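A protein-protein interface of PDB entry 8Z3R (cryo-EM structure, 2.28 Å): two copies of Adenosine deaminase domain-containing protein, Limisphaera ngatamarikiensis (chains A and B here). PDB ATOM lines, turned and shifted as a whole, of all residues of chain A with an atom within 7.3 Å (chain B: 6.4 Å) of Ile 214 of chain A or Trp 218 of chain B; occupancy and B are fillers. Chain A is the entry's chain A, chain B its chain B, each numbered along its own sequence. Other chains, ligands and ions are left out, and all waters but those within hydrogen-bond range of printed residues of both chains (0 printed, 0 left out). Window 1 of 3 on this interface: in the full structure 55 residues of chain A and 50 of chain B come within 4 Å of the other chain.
CG2 of Ile 214 of chain A touches CZ3 of Trp 218 of chain B (3.8 Å). O of Ala 227 of chain A touches CZ2 of Trp 218 of chain B, 3.9 Å away.
Ile 214 of chain A touches Trp 218 of chain B, but with the chains exchanged Trp 218 of chain A does not touch Ile 214 of chain B (4.3 Å). Positions printed for both chains: 213, 214, 215, 216, 217, 218, 219, 221 and 230. Of the 3 pairs that touch across the chains among the printed residues, none has its exchanged pair printed and touching as well.
Among the printed residues, 3 pairs touch across the chains. Among the printed residues, no Asp or Glu carboxylate lies within 4 Å of a Lys or Arg side-chain nitrogen of the other chain.
Ile 214 of chain A touches just one residue of chain B: Trp 218. Trp 218 of chain B touches just these residues of chain A: Arg 210, Ile 214 and Ala 227. Of the printed residues of chain B, Ala 227 of chain A touches Trp 218 (3.9 Å). Of the printed residues of chain B, Arg 210 of chain A touches Trp 218 (3.0 Å). The nearest residue of chain A that does not touch Trp 218 of chain B is Ala 230 of chain A (4.2 Å).
The guanidinium group (NH2) of Arg 210 of chain A lies close to the indole nitrogen (NE1) of Trp 218 of chain B, 3.1 Å away.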
ATOM      1  N   LEU A 207     -13.152  21.209  20.281  1.00  0.00           N
ATOM      2  CA  LEU A 207     -13.483  22.573  19.877  1.00  0.00           C
ATOM      3  C   LEU A 207     -12.357  23.541  20.230  1.00  0.00           C
ATOM      4  O   LEU A 207     -11.978  24.397  19.418  1.00  0.00           O
ATOM      5  CB  LEU A 207     -14.803  22.990  20.525  1.00  0.00           C
ATOM      6  CG  LEU A 207     -15.457  24.310  20.122  1.00  0.00           C
ATOM      7  CD1 LEU A 207     -16.938  24.180  20.341  1.00  0.00           C
ATOM      8  CD2 LEU A 207     -14.926  25.478  20.937  1.00  0.00           C
ATOM      9  N   LEU A 208     -11.807  23.416  21.440  1.00  0.00           N
ATOM     10  CA  LEU A 208     -10.705  24.285  21.839  1.00  0.00           C
ATOM     11  C   LEU A 208      -9.471  24.042  20.979  1.00  0.00           C
ATOM     12  O   LEU A 208      -8.772  24.991  20.604  1.00  0.00           O
ATOM     13  CB  LEU A 208     -10.380  24.074  23.318  1.00  0.00           C
ATOM     14  CG  LEU A 208     -11.367  24.656  24.329  1.00  0.00           C
ATOM     15  CD1 LEU A 208     -10.730  24.744  25.705  1.00  0.00           C
ATOM     16  CD2 LEU A 208     -11.852  26.023  23.880  1.00  0.00           C
ATOM     17  N   GLN A 209      -9.185  22.778  20.660  1.00  0.00           N
ATOM     18  CA  GLN A 209      -8.048  22.469  19.799  1.00  0.00           C
ATOM     19  C   GLN A 209      -8.230  23.068  18.411  1.00  0.00           C
ATOM     20  O   GLN A 209      -7.281  23.605  17.826  1.00  0.00           O
ATOM     21  CB  GLN A 209      -7.859  20.955  19.715  1.00  0.00           C
ATOM     22  CG  GLN A 209      -7.018  20.489  18.543  1.00  0.00           C
ATOM     23  CD  GLN A 209      -6.497  19.080  18.729  1.00  0.00           C
ATOM     24  OE1 GLN A 209      -6.995  18.136  18.116  1.00  0.00           O
ATOM     25  NE2 GLN A 209      -5.489  18.929  19.580  1.00  0.00           N
ATOM     26  N   ARG A 210      -9.446  22.985  17.869  1.00  0.00           N
ATOM     27  CA  ARG A 210      -9.725  23.572  16.564  1.00  0.00           C
ATOM     28  C   ARG A 210      -9.539  25.084  16.590  1.00  0.00           C
ATOM     29  O   ARG A 210      -8.946  25.660  15.669  1.00  0.00           O
ATOM     30  CB  ARG A 210     -11.145  23.203  16.137  1.00  0.00           C
ATOM     31  CG  ARG A 210     -11.559  23.677  14.762  1.00  0.00           C
ATOM     32  CD  ARG A 210     -12.965  23.190  14.460  1.00  0.00           C
ATOM     33  NE  ARG A 210     -13.420  23.573  13.132  1.00  0.00           N
ATOM     34  CZ  ARG A 210     -14.057  24.701  12.854  1.00  0.00           C
ATOM     35  NH1 ARG A 210     -14.323  25.595  13.792  1.00  0.00           N
ATOM     36  NH2 ARG A 210     -14.440  24.937  11.603  1.00  0.00           N
ATOM     37  N   ALA A 211     -10.034  25.740  17.642  1.00  0.00           N
ATOM     38  CA  ALA A 211      -9.851  27.184  17.758  1.00  0.00           C
ATOM     39  C   ALA A 211      -8.374  27.549  17.850  1.00  0.00           C
ATOM     40  O   ALA A 211      -7.923  28.511  17.217  1.00  0.00           O
ATOM     41  CB  ALA A 211     -10.610  27.714  18.973  1.00  0.00           C
ATOM     42  N   SER A 212      -7.606  26.787  18.633  1.00  0.00           N
ATOM     43  CA  SER A 212      -6.178  27.057  18.762  1.00  0.00           C
ATOM     44  C   SER A 212      -5.460  26.885  17.431  1.00  0.00           C
ATOM     45  O   SER A 212      -4.595  27.693  17.075  1.00  0.00           O
ATOM     46  CB  SER A 212      -5.567  26.144  19.823  1.00  0.00           C
ATOM     47  OG  SER A 212      -4.152  26.186  19.775  1.00  0.00           O
ATOM     48  N   ARG A 213      -5.800  25.836  16.680  1.00  0.00           N
ATOM     49  CA  ARG A 213      -5.164  25.620  15.384  1.00  0.00           C
ATOM     50  C   ARG A 213      -5.508  26.735  14.402  1.00  0.00           C
ATOM     51  O   ARG A 213      -4.634  27.213  13.666  1.00  0.00           O
ATOM     52  CB  ARG A 213      -5.570  24.259  14.823  1.00  0.00           C
ATOM     53  CG  ARG A 213      -4.745  23.105  15.365  1.00  0.00           C
ATOM     54  CD  ARG A 213      -5.354  21.765  14.994  1.00  0.00           C
ATOM     55  NE  ARG A 213      -4.717  20.666  15.709  1.00  0.00           N
ATOM     56  CZ  ARG A 213      -4.909  19.383  15.435  1.00  0.00           C
ATOM     57  NH1 ARG A 213      -5.721  18.998  14.464  1.00  0.00           N
ATOM     58  NH2 ARG A 213      -4.270  18.464  16.152  1.00  0.00           N
ATOM     59  N   ILE A 214      -6.774  27.163  14.374  1.00  0.00           N
ATOM     60  CA  ILE A 214      -7.160  28.260  13.488  1.00  0.00           C
ATOM     61  C   ILE A 214      -6.413  29.534  13.861  1.00  0.00           C
ATOM     62  O   ILE A 214      -5.941  30.271  12.987  1.00  0.00           O
ATOM     63  CB  ILE A 214      -8.685  28.469  13.511  1.00  0.00           C
ATOM     64  CG1 ILE A 214      -9.405  27.233  12.975  1.00  0.00           C
ATOM     65  CG2 ILE A 214      -9.068  29.694  12.700  1.00  0.00           C
ATOM     66  CD1 ILE A 214     -10.899  27.255  13.202  1.00  0.00           C
ATOM     67  N   ALA A 215      -6.296  29.819  15.160  1.00  0.00           N
ATOM     68  CA  ALA A 215      -5.523  30.981  15.583  1.00  0.00           C
ATOM     69  C   ALA A 215      -4.061  30.855  15.179  1.00  0.00           C
ATOM     70  O   ALA A 215      -3.430  31.850  14.809  1.00  0.00           O
ATOM     71  CB  ALA A 215      -5.643  31.177  17.093  1.00  0.00           C
ATOM     72  N   GLY A 216      -3.508  29.643  15.250  1.00  0.00           N
ATOM     73  CA  GLY A 216      -2.131  29.441  14.830  1.00  0.00           C
ATOM     74  C   GLY A 216      -1.929  29.693  13.349  1.00  0.00           C
ATOM     75  O   GLY A 216      -0.901  30.235  12.937  1.00  0.00           O
ATOM     76  N   ALA A 217      -2.899  29.298  12.529  1.00  0.00           N
ATOM     77  CA  ALA A 217      -2.846  29.545  11.091  1.00  0.00           C
ATOM     78  C   ALA A 217      -3.947  30.542  10.735  1.00  0.00           C
ATOM     79  O   ALA A 217      -5.040  30.169  10.308  1.00  0.00           O
ATOM     80  CB  ALA A 217      -2.987  28.241  10.306  1.00  0.00           C
ATOM     81  N   TRP A 218      -3.642  31.826  10.904  1.00  0.00           N
ATOM     82  CA  TRP A 218      -4.511  32.909  10.460  1.00  0.00           C
ATOM     83  C   TRP A 218      -3.905  33.718   9.328  1.00  0.00           C
ATOM     84  O   TRP A 218      -4.612  34.076   8.385  1.00  0.00           O
ATOM     85  CB  TRP A 218      -4.847  33.851  11.618  1.00  0.00           C
ATOM     86  CG  TRP A 218      -5.764  34.954  11.197  1.00  0.00           C
ATOM     87  CD1 TRP A 218      -5.516  36.292  11.253  1.00  0.00           C
ATOM     88  CD2 TRP A 218      -7.082  34.813  10.649  1.00  0.00           C
ATOM     89  NE1 TRP A 218      -6.595  36.994  10.774  1.00  0.00           N
ATOM     90  CE2 TRP A 218      -7.570  36.109  10.398  1.00  0.00           C
ATOM     91  CE3 TRP A 218      -7.895  33.717  10.350  1.00  0.00           C
ATOM     92  CZ2 TRP A 218      -8.833  36.338   9.861  1.00  0.00           C
ATOM     93  CZ3 TRP A 218      -9.148  33.947   9.817  1.00  0.00           C
ATOM     94  CH2 TRP A 218      -9.605  35.248   9.578  1.00  0.00           C
ATOM     95  N   GLU A 219      -2.612  34.017   9.405  1.00  0.00           N
ATOM     96  CA  GLU A 219      -1.878  34.459   8.234  1.00  0.00           C
ATOM     97  C   GLU A 219      -1.802  33.304   7.241  1.00  0.00           C
ATOM     98  O   GLU A 219      -2.346  32.220   7.473  1.00  0.00           O
ATOM     99  CB  GLU A 219      -0.485  34.947   8.628  1.00  0.00           C
ATOM    100  CG  GLU A 219      -0.479  36.202   9.488  1.00  0.00           C
ATOM    101  CD  GLU A 219      -0.988  37.425   8.751  1.00  0.00           C
ATOM    102  OE1 GLU A 219      -0.789  37.509   7.520  1.00  0.00           O
ATOM    103  OE2 GLU A 219      -1.582  38.307   9.405  1.00  0.00           O
ATOM    104  N   LEU A 221      -3.437  32.485   5.015  1.00  0.00           N
ATOM    105  CA  LEU A 221      -4.760  31.959   4.706  1.00  0.00           C
ATOM    106  C   LEU A 221      -5.165  32.255   3.261  1.00  0.00           C
ATOM    107  O   LEU A 221      -5.675  31.353   2.584  1.00  0.00           O
ATOM    108  CB  LEU A 221      -5.797  32.512   5.689  1.00  0.00           C
ATOM    109  CG  LEU A 221      -7.228  31.959   5.668  1.00  0.00           C
ATOM    110  CD1 LEU A 221      -7.850  32.113   7.041  1.00  0.00           C
ATOM    111  CD2 LEU A 221      -8.105  32.645   4.630  1.00  0.00           C
ATOM    112  N   ALA A 227     -10.221  26.662   2.723  1.00  0.00           N
ATOM    113  CA  ALA A 227     -10.228  27.247   4.060  1.00  0.00           C
ATOM    114  C   ALA A 227     -10.007  26.198   5.143  1.00  0.00           C
ATOM    115  O   ALA A 227      -9.338  26.468   6.146  1.00  0.00           O
ATOM    116  CB  ALA A 227     -11.541  27.991   4.298  1.00  0.00           C
ATOM    117  N   ASP A 228     -10.558  24.994   4.960  1.00  0.00           N
ATOM    118  CA  ASP A 228     -10.471  23.968   5.994  1.00  0.00           C
ATOM    119  C   ASP A 228      -9.035  23.570   6.303  1.00  0.00           C
ATOM    120  O   ASP A 228      -8.767  23.059   7.397  1.00  0.00           O
ATOM    121  CB  ASP A 228     -11.274  22.734   5.580  1.00  0.00           C
ATOM    122  CG  ASP A 228     -12.707  22.783   6.068  1.00  0.00           C
ATOM    123  OD1 ASP A 228     -13.498  21.898   5.681  1.00  0.00           O
ATOM    124  OD2 ASP A 228     -13.043  23.706   6.839  1.00  0.00           O
ATOM    125  N   LEU A 229      -8.103  23.806   5.377  1.00  0.00           N
ATOM    126  CA  LEU A 229      -6.698  23.526   5.641  1.00  0.00           C
ATOM    127  C   LEU A 229      -6.168  24.319   6.826  1.00  0.00           C
ATOM    128  O   LEU A 229      -5.157  23.928   7.418  1.00  0.00           O
ATOM    129  CB  LEU A 229      -5.861  23.826   4.397  1.00  0.00           C
ATOM    130  CG  LEU A 229      -6.115  22.935   3.181  1.00  0.00           C
ATOM    131  CD1 LEU A 229      -5.360  23.453   1.969  1.00  0.00           C
ATOM    132  CD2 LEU A 229      -5.728  21.497   3.481  1.00  0.00           C
ATOM    133  N   ALA A 230      -6.824  25.424   7.185  1.00  0.00           N
ATOM    134  CA  ALA A 230      -6.424  26.197   8.353  1.00  0.00           C
ATOM    135  C   ALA A 230      -6.682  25.467   9.663  1.00  0.00           C
ATOM    136  O   ALA A 230      -6.146  25.883  10.695  1.00  0.00           O
ATOM    137  CB  ALA A 230      -7.144  27.544   8.364  1.00  0.00           C
ATOM    138  N   THR A 231      -7.482  24.402   9.655  1.00  0.00           N
ATOM    139  CA  THR A 231      -7.767  23.637  10.861  1.00  0.00           C
ATOM    140  C   THR A 231      -6.803  22.473  11.057  1.00  0.00           C
ATOM    141  O   THR A 231      -6.960  21.706  12.011  1.00  0.00           O
ATOM    142  CB  THR A 231      -9.207  23.120  10.837  1.00  0.00           C
ATOM    143  OG1 THR A 231      -9.280  21.931  10.042  1.00  0.00           O
ATOM    144  CG2 THR A 231     -10.140  24.170  10.257  1.00  0.00           C
ATOM    145  N   TRP A 232      -5.817  22.324  10.178  1.00  0.00           N
ATOM    146  CA  TRP A 232      -4.830  21.267  10.318  1.00  0.00           C
ATOM    147  C   TRP A 232      -3.758  21.667  11.327  1.00  0.00           C
ATOM    148  O   TRP A 232      -3.558  22.847  11.630  1.00  0.00           O
ATOM    149  CB  TRP A 232      -4.184  20.951   8.968  1.00  0.00           C
ATOM    150  CG  TRP A 232      -5.040  20.117   8.065  1.00  0.00           C
ATOM    151  CD1 TRP A 232      -6.382  19.901   8.177  1.00  0.00           C
ATOM    152  CD2 TRP A 232      -4.610  19.377   6.917  1.00  0.00           C
ATOM    153  NE1 TRP A 232      -6.815  19.079   7.166  1.00  0.00           N
ATOM    154  CE2 TRP A 232      -5.746  18.742   6.380  1.00  0.00           C
ATOM    155  CE3 TRP A 232      -3.375  19.192   6.291  1.00  0.00           C
ATOM    156  CZ2 TRP A 232      -5.684  17.936   5.246  1.00  0.00           C
ATOM    157  CZ3 TRP A 232      -3.315  18.390   5.165  1.00  0.00           C
ATOM    158  CH2 TRP A 232      -4.462  17.773   4.655  1.00  0.00           C
ATOM    159  N   ARG A 620     -17.517  24.476  -1.165  1.00  0.00           N
ATOM    160  CA  ARG A 620     -17.766  23.986   0.188  1.00  0.00           C
ATOM    161  C   ARG A 620     -17.592  22.473   0.274  1.00  0.00           C
ATOM    162  O   ARG A 620     -16.944  21.963   1.199  1.00  0.00           O
ATOM    163  CB  ARG A 620     -19.166  24.388   0.647  1.00  0.00           C
ATOM    164  CG  ARG A 620     -19.262  25.795   1.207  1.00  0.00           C
ATOM    165  CD  ARG A 620     -20.699  26.134   1.570  1.00  0.00           C
ATOM    166  NE  ARG A 620     -20.929  27.571   1.675  1.00  0.00           N
ATOM    167  CZ  ARG A 620     -20.441  28.345   2.635  1.00  0.00           C
ATOM    168  NH1 ARG A 620     -19.701  27.852   3.615  1.00  0.00           N
ATOM    169  NH2 ARG A 620     -20.708  29.647   2.615  1.00  0.00           N
ATOM    170  N   ARG B 213     -14.303  35.706  18.466  1.00  0.00           N
ATOM    171  CA  ARG B 213     -15.044  36.266  17.340  1.00  0.00           C
ATOM    172  C   ARG B 213     -14.805  35.467  16.064  1.00  0.00           C
ATOM    173  O   ARG B 213     -15.742  35.218  15.294  1.00  0.00           O
ATOM    174  CB  ARG B 213     -14.668  37.734  17.143  1.00  0.00           C
ATOM    175  CG  ARG B 213     -15.510  38.693  17.965  1.00  0.00           C
ATOM    176  CD  ARG B 213     -14.746  39.958  18.308  1.00  0.00           C
ATOM    177  NE  ARG B 213     -15.560  40.885  19.085  1.00  0.00           N
ATOM    178  CZ  ARG B 213     -15.260  42.162  19.281  1.00  0.00           C
ATOM    179  NH1 ARG B 213     -14.167  42.702  18.767  1.00  0.00           N
ATOM    180  NH2 ARG B 213     -16.077  42.915  20.011  1.00  0.00           N
ATOM    181  N   ILE B 214     -13.557  35.053  15.822  1.00  0.00           N
ATOM    182  CA  ILE B 214     -13.273  34.223  14.653  1.00  0.00           C
ATOM    183  C   ILE B 214     -14.024  32.901  14.742  1.00  0.00           C
ATOM    184  O   ILE B 214     -14.583  32.420  13.749  1.00  0.00           O
ATOM    185  CB  ILE B 214     -11.757  34.005  14.492  1.00  0.00           C
ATOM    186  CG1 ILE B 214     -11.048  35.335  14.238  1.00  0.00           C
ATOM    187  CG2 ILE B 214     -11.475  33.034  13.361  1.00  0.00           C
ATOM    188  CD1 ILE B 214      -9.543  35.247  14.326  1.00  0.00           C
ATOM    189  N   ALA B 215     -14.051  32.292  15.930  1.00  0.00           N
ATOM    190  CA  ALA B 215     -14.808  31.056  16.102  1.00  0.00           C
ATOM    191  C   ALA B 215     -16.292  31.280  15.843  1.00  0.00           C
ATOM    192  O   ALA B 215     -16.962  30.432  15.244  1.00  0.00           O
ATOM    193  CB  ALA B 215     -14.587  30.493  17.506  1.00  0.00           C
ATOM    194  N   GLY B 216     -16.822  32.417  16.292  1.00  0.00           N
ATOM    195  CA  GLY B 216     -18.225  32.714  16.058  1.00  0.00           C
ATOM    196  C   GLY B 216     -18.549  32.895  14.589  1.00  0.00           C
ATOM    197  O   GLY B 216     -19.616  32.485  14.125  1.00  0.00           O
ATOM    198  N   ALA B 217     -17.641  33.514  13.840  1.00  0.00           N
ATOM    199  CA  ALA B 217     -17.825  33.718  12.405  1.00  0.00           C
ATOM    200  C   ALA B 217     -16.760  32.917  11.661  1.00  0.00           C
ATOM    201  O   ALA B 217     -15.701  33.431  11.300  1.00  0.00           O
ATOM    202  CB  ALA B 217     -17.763  35.204  12.055  1.00  0.00           C
ATOM    203  N   TRP B 218     -17.055  31.641  11.425  1.00  0.00           N
ATOM    204  CA  TRP B 218     -16.228  30.782  10.586  1.00  0.00           C
ATOM    205  C   TRP B 218     -16.916  30.367   9.301  1.00  0.00           C
ATOM    206  O   TRP B 218     -16.285  30.367   8.241  1.00  0.00           O
ATOM    207  CB  TRP B 218     -15.802  29.524  11.345  1.00  0.00           C
ATOM    208  CG  TRP B 218     -14.855  28.684  10.554  1.00  0.00           C
ATOM    209  CD1 TRP B 218     -15.092  27.442  10.049  1.00  0.00           C
ATOM    210  CD2 TRP B 218     -13.528  29.037  10.147  1.00  0.00           C
ATOM    211  NE1 TRP B 218     -13.989  26.991   9.366  1.00  0.00           N
ATOM    212  CE2 TRP B 218     -13.015  27.952   9.411  1.00  0.00           C
ATOM    213  CE3 TRP B 218     -12.721  30.162  10.341  1.00  0.00           C
ATOM    214  CZ2 TRP B 218     -11.734  27.958   8.868  1.00  0.00           C
ATOM    215  CZ3 TRP B 218     -11.449  30.166   9.800  1.00  0.00           C
ATOM    216  CH2 TRP B 218     -10.968  29.071   9.074  1.00  0.00           C
ATOM    217  N   GLU B 219     -18.195  30.012   9.367  1.00  0.00           N
ATOM    218  CA  GLU B 219     -18.980  29.883   8.156  1.00  0.00           C
ATOM    219  C   GLU B 219     -19.103  31.252   7.490  1.00  0.00           C
ATOM    220  O   GLU B 219     -18.586  32.258   7.984  1.00  0.00           O
ATOM    221  CB  GLU B 219     -20.361  29.307   8.464  1.00  0.00           C
ATOM    222  CG  GLU B 219     -20.344  27.869   8.951  1.00  0.00           C
ATOM    223  CD  GLU B 219     -20.050  27.762  10.435  1.00  0.00           C
ATOM    224  OE1 GLU B 219     -19.921  28.815  11.094  1.00  0.00           O
ATOM    225  OE2 GLU B 219     -19.949  26.626  10.941  1.00  0.00           O
ATOM    226  N   MET B 220     -19.775  31.276   6.338  1.00  0.00           N
ATOM    227  CA  MET B 220     -19.987  32.487   5.545  1.00  0.00           C
ATOM    228  C   MET B 220     -18.716  33.318   5.370  1.00  0.00           C
ATOM    229  O   MET B 220     -18.785  34.519   5.096  1.00  0.00           O
ATOM    230  CB  MET B 220     -21.137  33.332   6.129  1.00  0.00           C
ATOM    231  CG  MET B 220     -20.997  33.868   7.560  1.00  0.00           C
ATOM    232  SD  MET B 220     -19.968  35.329   7.775  1.00  0.00           S
ATOM    233  CE  MET B 220     -21.008  36.558   7.010  1.00  0.00           C
ATOM    234  N   LEU B 221     -17.554  32.678   5.488  1.00  0.00           N
ATOM    235  CA  LEU B 221     -16.266  33.327   5.269  1.00  0.00           C
ATOM    236  C   LEU B 221     -15.941  33.425   3.779  1.00  0.00           C
ATOM    237  O   LEU B 221     -15.393  34.449   3.348  1.00  0.00           O
ATOM    238  CB  LEU B 221     -15.154  32.598   6.031  1.00  0.00           C
ATOM    239  CG  LEU B 221     -13.799  33.305   6.095  1.00  0.00           C
ATOM    240  CD1 LEU B 221     -13.962  34.700   6.665  1.00  0.00           C
ATOM    241  CD2 LEU B 221     -12.808  32.504   6.925  1.00  0.00           C
ATOM    242  N   PRO B 222     -16.228  32.403   2.960  1.00  0.00           N
ATOM    243  CA  PRO B 222     -16.051  32.582   1.507  1.00  0.00           C
ATOM    244  C   PRO B 222     -16.803  33.774   0.938  1.00  0.00           C
ATOM    245  O   PRO B 222     -16.282  34.450   0.043  1.00  0.00           O
ATOM    246  CB  PRO B 222     -16.577  31.267   0.914  1.00  0.00           C
ATOM    247  CG  PRO B 222     -16.733  30.315   2.049  1.00  0.00           C
ATOM    248  CD  PRO B 222     -16.309  30.973   3.315  1.00  0.00           C
ATOM    249  N   ALA B 230     -14.015  38.850   9.594  1.00  0.00           N
ATOM    250  CA  ALA B 230     -14.352  37.786  10.530  1.00  0.00           C
ATOM    251  C   ALA B 230     -14.003  38.143  11.969  1.00  0.00           C
ATOM    252  O   ALA B 230     -14.537  37.523  12.894  1.00  0.00           O
ATOM    253  CB  ALA B 230     -13.646  36.490  10.132  1.00  0.00           C
